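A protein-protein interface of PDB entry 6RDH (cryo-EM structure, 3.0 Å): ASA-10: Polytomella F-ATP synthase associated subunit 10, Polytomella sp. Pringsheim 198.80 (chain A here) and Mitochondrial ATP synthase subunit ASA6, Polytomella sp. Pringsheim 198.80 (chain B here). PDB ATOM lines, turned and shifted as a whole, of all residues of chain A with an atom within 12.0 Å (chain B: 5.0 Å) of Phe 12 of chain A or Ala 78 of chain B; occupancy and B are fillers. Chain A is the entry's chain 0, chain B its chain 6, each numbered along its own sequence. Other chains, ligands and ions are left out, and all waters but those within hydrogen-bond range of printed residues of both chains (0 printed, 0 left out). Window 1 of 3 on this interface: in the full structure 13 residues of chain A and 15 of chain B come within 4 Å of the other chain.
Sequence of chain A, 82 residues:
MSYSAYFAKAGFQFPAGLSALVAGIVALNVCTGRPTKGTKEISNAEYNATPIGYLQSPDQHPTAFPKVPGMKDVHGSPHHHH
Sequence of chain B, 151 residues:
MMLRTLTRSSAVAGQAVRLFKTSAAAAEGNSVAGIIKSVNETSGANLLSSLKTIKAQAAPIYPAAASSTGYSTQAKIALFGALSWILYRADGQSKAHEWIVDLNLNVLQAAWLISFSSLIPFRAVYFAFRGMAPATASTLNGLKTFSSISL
The backbone NH (N) of Phe 14 of chain A sits close to the side-chain amide nitrogen (NE2) of Gln 74 of chain B, at 3.0 Å.
Among the printed residues, merely in contact across the chains: Phe 12 of chain A with Ser 72 of chain B (3.7 Å), Phe 12 of chain A with Gln 74 of chain B (3.8 Å), Phe 12 of chain A with Ala 75 of chain B (3.7 Å), Phe 12 of chain A with Ala 78 of chain B (3.7 Å), Gln 13 of chain A with Gln 74 of chain B (3.6 Å), Phe 14 of chain A with Ile 77 of chain B (3.8 Å) and Phe 14 of chain A with Ala 78 of chain B (3.8 Å).
Phe 12 of chain A touches just these residues of chain B: Ser 72, Gln 74, Ala 75 and Ala 78. Ser 72 of chain B touches just one residue of chain A: Phe 12 (3.7 Å). Of the printed residues of chain A, Gln 74 of chain B touches Phe 12, Gln 13 and Phe 14. Of chain A, only Phe 14 (3.8 Å) comes within 4 Å of Ile 77 of chain B. No residue of chain A comes within 4 Å of Leu 79 of chain B. No residue of chain A comes within 4 Å of Gly 81 of chain B. Printed residues of chain B within 4 Å of Gln 13 of chain A: Gln 74 (3.6 Å). Of the printed residues of chain B, Phe 14 of chain A touches Gln 74 (3.0 Å), Ile 77 (3.8 Å) and Ala 78 (3.8 Å). Gly 11 of chain A touches none of the printed residues of chain B. Ala 10 of chain A touches none of the printed residues of chain B.
Of the 15 printed residues of chain A, 3 touch a printed residue of chain B. Hydrophobic or aromatic side chains of chain A within 4 Å of the printed part of chain B: Phe 12 and Phe 14. Among the printed residues, 8 pairs touch across the chains. Among the printed residues, no Asp or Glu carboxylate lies within 4 Å of a Lys or Arg side-chain nitrogen of the other chain.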
ATOM      1  N   TYR A   6       5.146 -23.333  13.823  1.00  0.00           N
ATOM      2  CA  TYR A   6       4.737 -22.488  12.715  1.00  0.00           C
ATOM      3  C   TYR A   6       4.960 -21.024  13.033  1.00  0.00           C
ATOM      4  O   TYR A   6       5.263 -20.238  12.134  1.00  0.00           O
ATOM      5  CB  TYR A   6       3.274 -22.747  12.383  1.00  0.00           C
ATOM      6  CG  TYR A   6       2.653 -21.737  11.469  1.00  0.00           C
ATOM      7  CD1 TYR A   6       3.087 -21.594  10.171  1.00  0.00           C
ATOM      8  CD2 TYR A   6       1.624 -20.935  11.905  1.00  0.00           C
ATOM      9  CE1 TYR A   6       2.517 -20.671   9.340  1.00  0.00           C
ATOM     10  CE2 TYR A   6       1.050 -20.018  11.086  1.00  0.00           C
ATOM     11  CZ  TYR A   6       1.496 -19.888   9.805  1.00  0.00           C
ATOM     12  OH  TYR A   6       0.918 -18.962   8.976  1.00  0.00           O
ATOM     13  N   PHE A   7       4.837 -20.644  14.301  1.00  0.00           N
ATOM     14  CA  PHE A   7       5.060 -19.260  14.680  1.00  0.00           C
ATOM     15  C   PHE A   7       6.525 -18.942  14.874  1.00  0.00           C
ATOM     16  O   PHE A   7       6.909 -17.776  14.762  1.00  0.00           O
ATOM     17  CB  PHE A   7       4.289 -18.935  15.948  1.00  0.00           C
ATOM     18  CG  PHE A   7       2.829 -19.092  15.794  1.00  0.00           C
ATOM     19  CD1 PHE A   7       2.143 -18.365  14.845  1.00  0.00           C
ATOM     20  CD2 PHE A   7       2.140 -19.970  16.583  1.00  0.00           C
ATOM     21  CE1 PHE A   7       0.805 -18.524  14.696  1.00  0.00           C
ATOM     22  CE2 PHE A   7       0.807 -20.129  16.432  1.00  0.00           C
ATOM     23  CZ  PHE A   7       0.138 -19.406  15.496  1.00  0.00           C
ATOM     24  N   ALA A   8       7.351 -19.948  15.141  1.00  0.00           N
ATOM     25  CA  ALA A   8       8.782 -19.720  15.215  1.00  0.00           C
ATOM     26  C   ALA A   8       9.396 -19.484  13.844  1.00  0.00           C
ATOM     27  O   ALA A   8      10.525 -18.993  13.764  1.00  0.00           O
ATOM     28  CB  ALA A   8       9.459 -20.899  15.901  1.00  0.00           C
ATOM     29  N   LYS A   9       8.684 -19.824  12.771  1.00  0.00           N
ATOM     30  CA  LYS A   9       9.199 -19.595  11.428  1.00  0.00           C
ATOM     31  C   LYS A   9       9.230 -18.112  11.099  1.00  0.00           C
ATOM     32  O   LYS A   9      10.226 -17.603  10.580  1.00  0.00           O
ATOM     33  CB  LYS A   9       8.355 -20.347  10.404  1.00  0.00           C
ATOM     34  CG  LYS A   9       8.518 -21.846  10.461  1.00  0.00           C
ATOM     35  CD  LYS A   9       7.746 -22.510   9.340  1.00  0.00           C
ATOM     36  CE  LYS A   9       7.817 -24.015   9.439  1.00  0.00           C
ATOM     37  NZ  LYS A   9       7.137 -24.648   8.294  1.00  0.00           N
ATOM     38  N   ALA A  10       8.143 -17.407  11.376  1.00  0.00           N
ATOM     39  CA  ALA A  10       8.119 -15.966  11.188  1.00  0.00           C
ATOM     40  C   ALA A  10       8.883 -15.320  12.330  1.00  0.00           C
ATOM     41  O   ALA A  10       8.542 -15.517  13.500  1.00  0.00           O
ATOM     42  CB  ALA A  10       6.685 -15.453  11.131  1.00  0.00           C
ATOM     43  N   GLY A  11       9.918 -14.562  12.001  1.00  0.00           N
ATOM     44  CA  GLY A  11      10.754 -14.000  13.036  1.00  0.00           C
ATOM     45  C   GLY A  11      10.196 -12.722  13.614  1.00  0.00           C
ATOM     46  O   GLY A  11       8.983 -12.582  13.782  1.00  0.00           O
ATOM     47  N   PHE A  12      11.077 -11.789  13.943  1.00  0.00           N
ATOM     48  CA  PHE A  12      10.636 -10.466  14.335  1.00  0.00           C
ATOM     49  C   PHE A  12      10.063  -9.745  13.129  1.00  0.00           C
ATOM     50  O   PHE A  12      10.500  -9.935  11.994  1.00  0.00           O
ATOM     51  CB  PHE A  12      11.796  -9.671  14.925  1.00  0.00           C
ATOM     52  CG  PHE A  12      11.422  -8.302  15.397  1.00  0.00           C
ATOM     53  CD1 PHE A  12      10.819  -8.125  16.619  1.00  0.00           C
ATOM     54  CD2 PHE A  12      11.679  -7.193  14.615  1.00  0.00           C
ATOM     55  CE1 PHE A  12      10.479  -6.870  17.051  1.00  0.00           C
ATOM     56  CE2 PHE A  12      11.336  -5.942  15.042  1.00  0.00           C
ATOM     57  CZ  PHE A  12      10.740  -5.778  16.256  1.00  0.00           C
ATOM     58  N   GLN A  13       9.066  -8.911  13.387  1.00  0.00           N
ATOM     59  CA  GLN A  13       8.404  -8.181  12.329  1.00  0.00           C
ATOM     60  C   GLN A  13       7.820  -6.927  12.955  1.00  0.00           C
ATOM     61  O   GLN A  13       7.277  -6.977  14.060  1.00  0.00           O
ATOM     62  CB  GLN A  13       7.345  -9.067  11.673  1.00  0.00           C
ATOM     63  CG  GLN A  13       6.834  -8.594  10.352  1.00  0.00           C
ATOM     64  CD  GLN A  13       6.010  -9.659   9.674  1.00  0.00           C
ATOM     65  OE1 GLN A  13       5.786 -10.728  10.234  1.00  0.00           O
ATOM     66  NE2 GLN A  13       5.571  -9.382   8.456  1.00  0.00           N
ATOM     67  N   PHE A  14       7.969  -5.806  12.259  1.00  0.00           N
ATOM     68  CA  PHE A  14       7.568  -4.513  12.777  1.00  0.00           C
ATOM     69  C   PHE A  14       6.051  -4.403  12.839  1.00  0.00           C
ATOM     70  O   PHE A  14       5.344  -5.207  12.232  1.00  0.00           O
ATOM     71  CB  PHE A  14       8.134  -3.408  11.894  1.00  0.00           C
ATOM     72  CG  PHE A  14       9.554  -3.077  12.192  1.00  0.00           C
ATOM     73  CD1 PHE A  14       9.978  -2.932  13.493  1.00  0.00           C
ATOM     74  CD2 PHE A  14      10.467  -2.916  11.175  1.00  0.00           C
ATOM     75  CE1 PHE A  14      11.281  -2.632  13.773  1.00  0.00           C
ATOM     76  CE2 PHE A  14      11.771  -2.619  11.452  1.00  0.00           C
ATOM     77  CZ  PHE A  14      12.176  -2.475  12.753  1.00  0.00           C
ATOM     78  N   PRO A  15       5.527  -3.442  13.608  1.00  0.00           N
ATOM     79  CA  PRO A  15       4.105  -3.126  13.515  1.00  0.00           C
ATOM     80  C   PRO A  15       3.718  -2.711  12.109  1.00  0.00           C
ATOM     81  O   PRO A  15       4.529  -2.195  11.341  1.00  0.00           O
ATOM     82  CB  PRO A  15       3.942  -1.981  14.507  1.00  0.00           C
ATOM     83  CG  PRO A  15       4.898  -2.299  15.533  1.00  0.00           C
ATOM     84  CD  PRO A  15       6.092  -2.889  14.847  1.00  0.00           C
ATOM     85  N   ALA A  16       2.465  -2.956  11.770  1.00  0.00           N
ATOM     86  CA  ALA A  16       2.077  -3.042  10.375  1.00  0.00           C
ATOM     87  C   ALA A  16       1.910  -1.704   9.688  1.00  0.00           C
ATOM     88  O   ALA A  16       1.438  -1.683   8.551  1.00  0.00           O
ATOM     89  CB  ALA A  16       0.782  -3.826  10.244  1.00  0.00           C
ATOM     90  N   GLY A  17       2.244  -0.598  10.325  1.00  0.00           N
ATOM     91  CA  GLY A  17       2.268   0.650   9.599  1.00  0.00           C
ATOM     92  C   GLY A  17       3.375   1.562  10.058  1.00  0.00           C
ATOM     93  O   GLY A  17       3.272   2.776   9.893  1.00  0.00           O
ATOM     94  N   LEU A  18       4.435   0.985  10.628  1.00  0.00           N
ATOM     95  CA  LEU A  18       5.457   1.754  11.328  1.00  0.00           C
ATOM     96  C   LEU A  18       6.233   2.673  10.410  1.00  0.00           C
ATOM     97  O   LEU A  18       6.742   3.698  10.869  1.00  0.00           O
ATOM     98  CB  LEU A  18       6.428   0.814  12.019  1.00  0.00           C
ATOM     99  CG  LEU A  18       7.218   1.402  13.171  1.00  0.00           C
ATOM    100  CD1 LEU A  18       6.273   1.867  14.238  1.00  0.00           C
ATOM    101  CD2 LEU A  18       8.167   0.380  13.712  1.00  0.00           C
ATOM    102  N   SER A  19       6.321   2.341   9.127  1.00  0.00           N
ATOM    103  CA  SER A  19       6.967   3.228   8.179  1.00  0.00           C
ATOM    104  C   SER A  19       6.199   4.524   8.016  1.00  0.00           C
ATOM    105  O   SER A  19       6.812   5.568   7.808  1.00  0.00           O
ATOM    106  CB  SER A  19       7.129   2.523   6.844  1.00  0.00           C
ATOM    107  OG  SER A  19       5.870   2.199   6.291  1.00  0.00           O
ATOM    108  N   VAL A  22       7.255   6.567  11.249  1.00  0.00           N
ATOM    109  CA  VAL A  22       8.615   7.075  11.136  1.00  0.00           C
ATOM    110  C   VAL A  22       8.708   8.123  10.035  1.00  0.00           C
ATOM    111  O   VAL A  22       9.373   9.150  10.208  1.00  0.00           O
ATOM    112  CB  VAL A  22       9.582   5.900  10.922  1.00  0.00           C
ATOM    113  CG1 VAL A  22      10.994   6.379  10.714  1.00  0.00           C
ATOM    114  CG2 VAL A  22       9.535   4.984  12.111  1.00  0.00           C
ATOM    115  N   SER B  72      16.451 -11.941  11.183  1.00  0.00           N
ATOM    116  CA  SER B  72      15.965 -11.500   9.882  1.00  0.00           C
ATOM    117  C   SER B  72      16.201 -10.016   9.629  1.00  0.00           C
ATOM    118  O   SER B  72      16.732  -9.309  10.489  1.00  0.00           O
ATOM    119  CB  SER B  72      14.476 -11.799   9.763  1.00  0.00           C
ATOM    120  OG  SER B  72      13.740 -11.022  10.679  1.00  0.00           O
ATOM    121  N   GLN B  74      14.265  -7.377   9.369  1.00  0.00           N
ATOM    122  CA  GLN B  74      13.601  -6.398  10.211  1.00  0.00           C
ATOM    123  C   GLN B  74      14.095  -6.471  11.642  1.00  0.00           C
ATOM    124  O   GLN B  74      14.153  -5.444  12.315  1.00  0.00           O
ATOM    125  CB  GLN B  74      12.097  -6.591  10.126  1.00  0.00           C
ATOM    126  CG  GLN B  74      11.610  -6.450   8.715  1.00  0.00           C
ATOM    127  CD  GLN B  74      10.128  -6.483   8.611  1.00  0.00           C
ATOM    128  OE1 GLN B  74       9.576  -6.952   7.625  1.00  0.00           O
ATOM    129  NE2 GLN B  74       9.460  -5.990   9.631  1.00  0.00           N
ATOM    130  N   ALA B  75      14.505  -7.648  12.105  1.00  0.00           N
ATOM    131  CA  ALA B  75      15.163  -7.735  13.401  1.00  0.00           C
ATOM    132  C   ALA B  75      16.532  -7.081  13.377  1.00  0.00           C
ATOM    133  O   ALA B  75      16.952  -6.491  14.378  1.00  0.00           O
ATOM    134  CB  ALA B  75      15.296  -9.189  13.831  1.00  0.00           C
ATOM    135  N   LYS B  76      17.235  -7.160  12.249  1.00  0.00           N
ATOM    136  CA  LYS B  76      18.516  -6.476  12.143  1.00  0.00           C
ATOM    137  C   LYS B  76      18.328  -4.971  12.073  1.00  0.00           C
ATOM    138  O   LYS B  76      19.110  -4.228  12.670  1.00  0.00           O
ATOM    139  CB  LYS B  76      19.290  -6.966  10.924  1.00  0.00           C
ATOM    140  CG  LYS B  76      19.886  -8.361  11.053  1.00  0.00           C
ATOM    141  CD  LYS B  76      20.814  -8.666   9.889  1.00  0.00           C
ATOM    142  CE  LYS B  76      20.147  -8.389   8.550  1.00  0.00           C
ATOM    143  NZ  LYS B  76      21.059  -8.532   7.386  1.00  0.00           N
ATOM    144  N   ILE B  77      17.297  -4.506  11.355  1.00  0.00           N
ATOM    145  CA  ILE B  77      16.972  -3.080  11.337  1.00  0.00           C
ATOM    146  C   ILE B  77      16.591  -2.603  12.733  1.00  0.00           C
ATOM    147  O   ILE B  77      17.012  -1.529  13.164  1.00  0.00           O
ATOM    148  CB  ILE B  77      15.857  -2.792  10.313  1.00  0.00           C
ATOM    149  CG1 ILE B  77      16.390  -2.872   8.893  1.00  0.00           C
ATOM    150  CG2 ILE B  77      15.276  -1.409  10.488  1.00  0.00           C
ATOM    151  CD1 ILE B  77      15.302  -2.819   7.849  1.00  0.00           C
ATOM    152  N   ALA B  78      15.863  -3.427  13.485  1.00  0.00           N
ATOM    153  CA  ALA B  78      15.472  -3.061  14.842  1.00  0.00           C
ATOM    154  C   ALA B  78      16.673  -2.968  15.772  1.00  0.00           C
ATOM    155  O   ALA B  78      16.804  -2.001  16.524  1.00  0.00           O
ATOM    156  CB  ALA B  78      14.464  -4.065  15.386  1.00  0.00           C
ATOM    157  N   LEU B  79      17.578  -3.946  15.720  1.00  0.00           N
ATOM    158  CA  LEU B  79      18.723  -3.910  16.623  1.00  0.00           C
ATOM    159  C   LEU B  79      19.736  -2.847  16.216  1.00  0.00           C
ATOM    160  O   LEU B  79      20.328  -2.197  17.087  1.00  0.00           O
ATOM    161  CB  LEU B  79      19.382  -5.282  16.696  1.00  0.00           C
ATOM    162  CG  LEU B  79      18.681  -6.278  17.619  1.00  0.00           C
ATOM    163  CD1 LEU B  79      19.438  -7.592  17.669  1.00  0.00           C
ATOM    164  CD2 LEU B  79      18.509  -5.704  19.013  1.00  0.00           C
ATOM    165  N   PHE B  80      19.915  -2.616  14.914  1.00  0.00           N
ATOM    166  CA  PHE B  80      20.817  -1.561  14.481  1.00  0.00           C
ATOM    167  C   PHE B  80      20.240  -0.190  14.778  1.00  0.00           C
ATOM    168  O   PHE B  80      20.975   0.713  15.179  1.00  0.00           O
ATOM    169  CB  PHE B  80      21.121  -1.686  12.994  1.00  0.00           C
ATOM    170  CG  PHE B  80      22.122  -0.687  12.503  1.00  0.00           C
ATOM    171  CD1 PHE B  80      21.726   0.394  11.733  1.00  0.00           C
ATOM    172  CD2 PHE B  80      23.462  -0.821  12.820  1.00  0.00           C
ATOM    173  CE1 PHE B  80      22.654   1.321  11.286  1.00  0.00           C
ATOM    174  CE2 PHE B  80      24.392   0.102  12.374  1.00  0.00           C
ATOM    175  CZ  PHE B  80      23.987   1.171  11.608  1.00  0.00           C
ATOM    176  N   GLY B  81      18.930  -0.014  14.608  1.00  0.00           N
ATOM    177  CA  GLY B  81      18.311   1.250  14.944  1.00  0.00           C
ATOM    178  C   GLY B  81      18.282   1.515  16.430  1.00  0.00           C
ATOM    179  O   GLY B  81      18.442   2.656  16.853  1.00  0.00           O
ATOM    180  N   ALA B  82      18.122   0.469  17.241  1.00  0.00           N
ATOM    181  CA  ALA B  82      18.161   0.644  18.686  1.00  0.00           C
ATOM    182  C   ALA B  82      19.559   1.001  19.154  1.00  0.00           C
ATOM    183  O   ALA B  82      19.721   1.887  19.999  1.00  0.00           O
ATOM    184  CB  ALA B  82      17.680  -0.620  19.387  1.00  0.00           C
ATOM    185  N   LEU B  83      20.582   0.346  18.601  1.00  0.00           N
ATOM    186  CA  LEU B  83      21.951   0.685  18.972  1.00  0.00           C
ATOM    187  C   LEU B  83      22.343   2.063  18.462  1.00  0.00           C
ATOM    188  O   LEU B  83      23.028   2.811  19.163  1.00  0.00           O
ATOM    189  CB  LEU B  83      22.915  -0.364  18.442  1.00  0.00           C
ATOM    190  CG  LEU B  83      24.276  -0.321  19.114  1.00  0.00           C
ATOM    191  CD1 LEU B  83      24.118  -0.610  20.587  1.00  0.00           C
ATOM    192  CD2 LEU B  83      25.206  -1.317  18.462  1.00  0.00           C
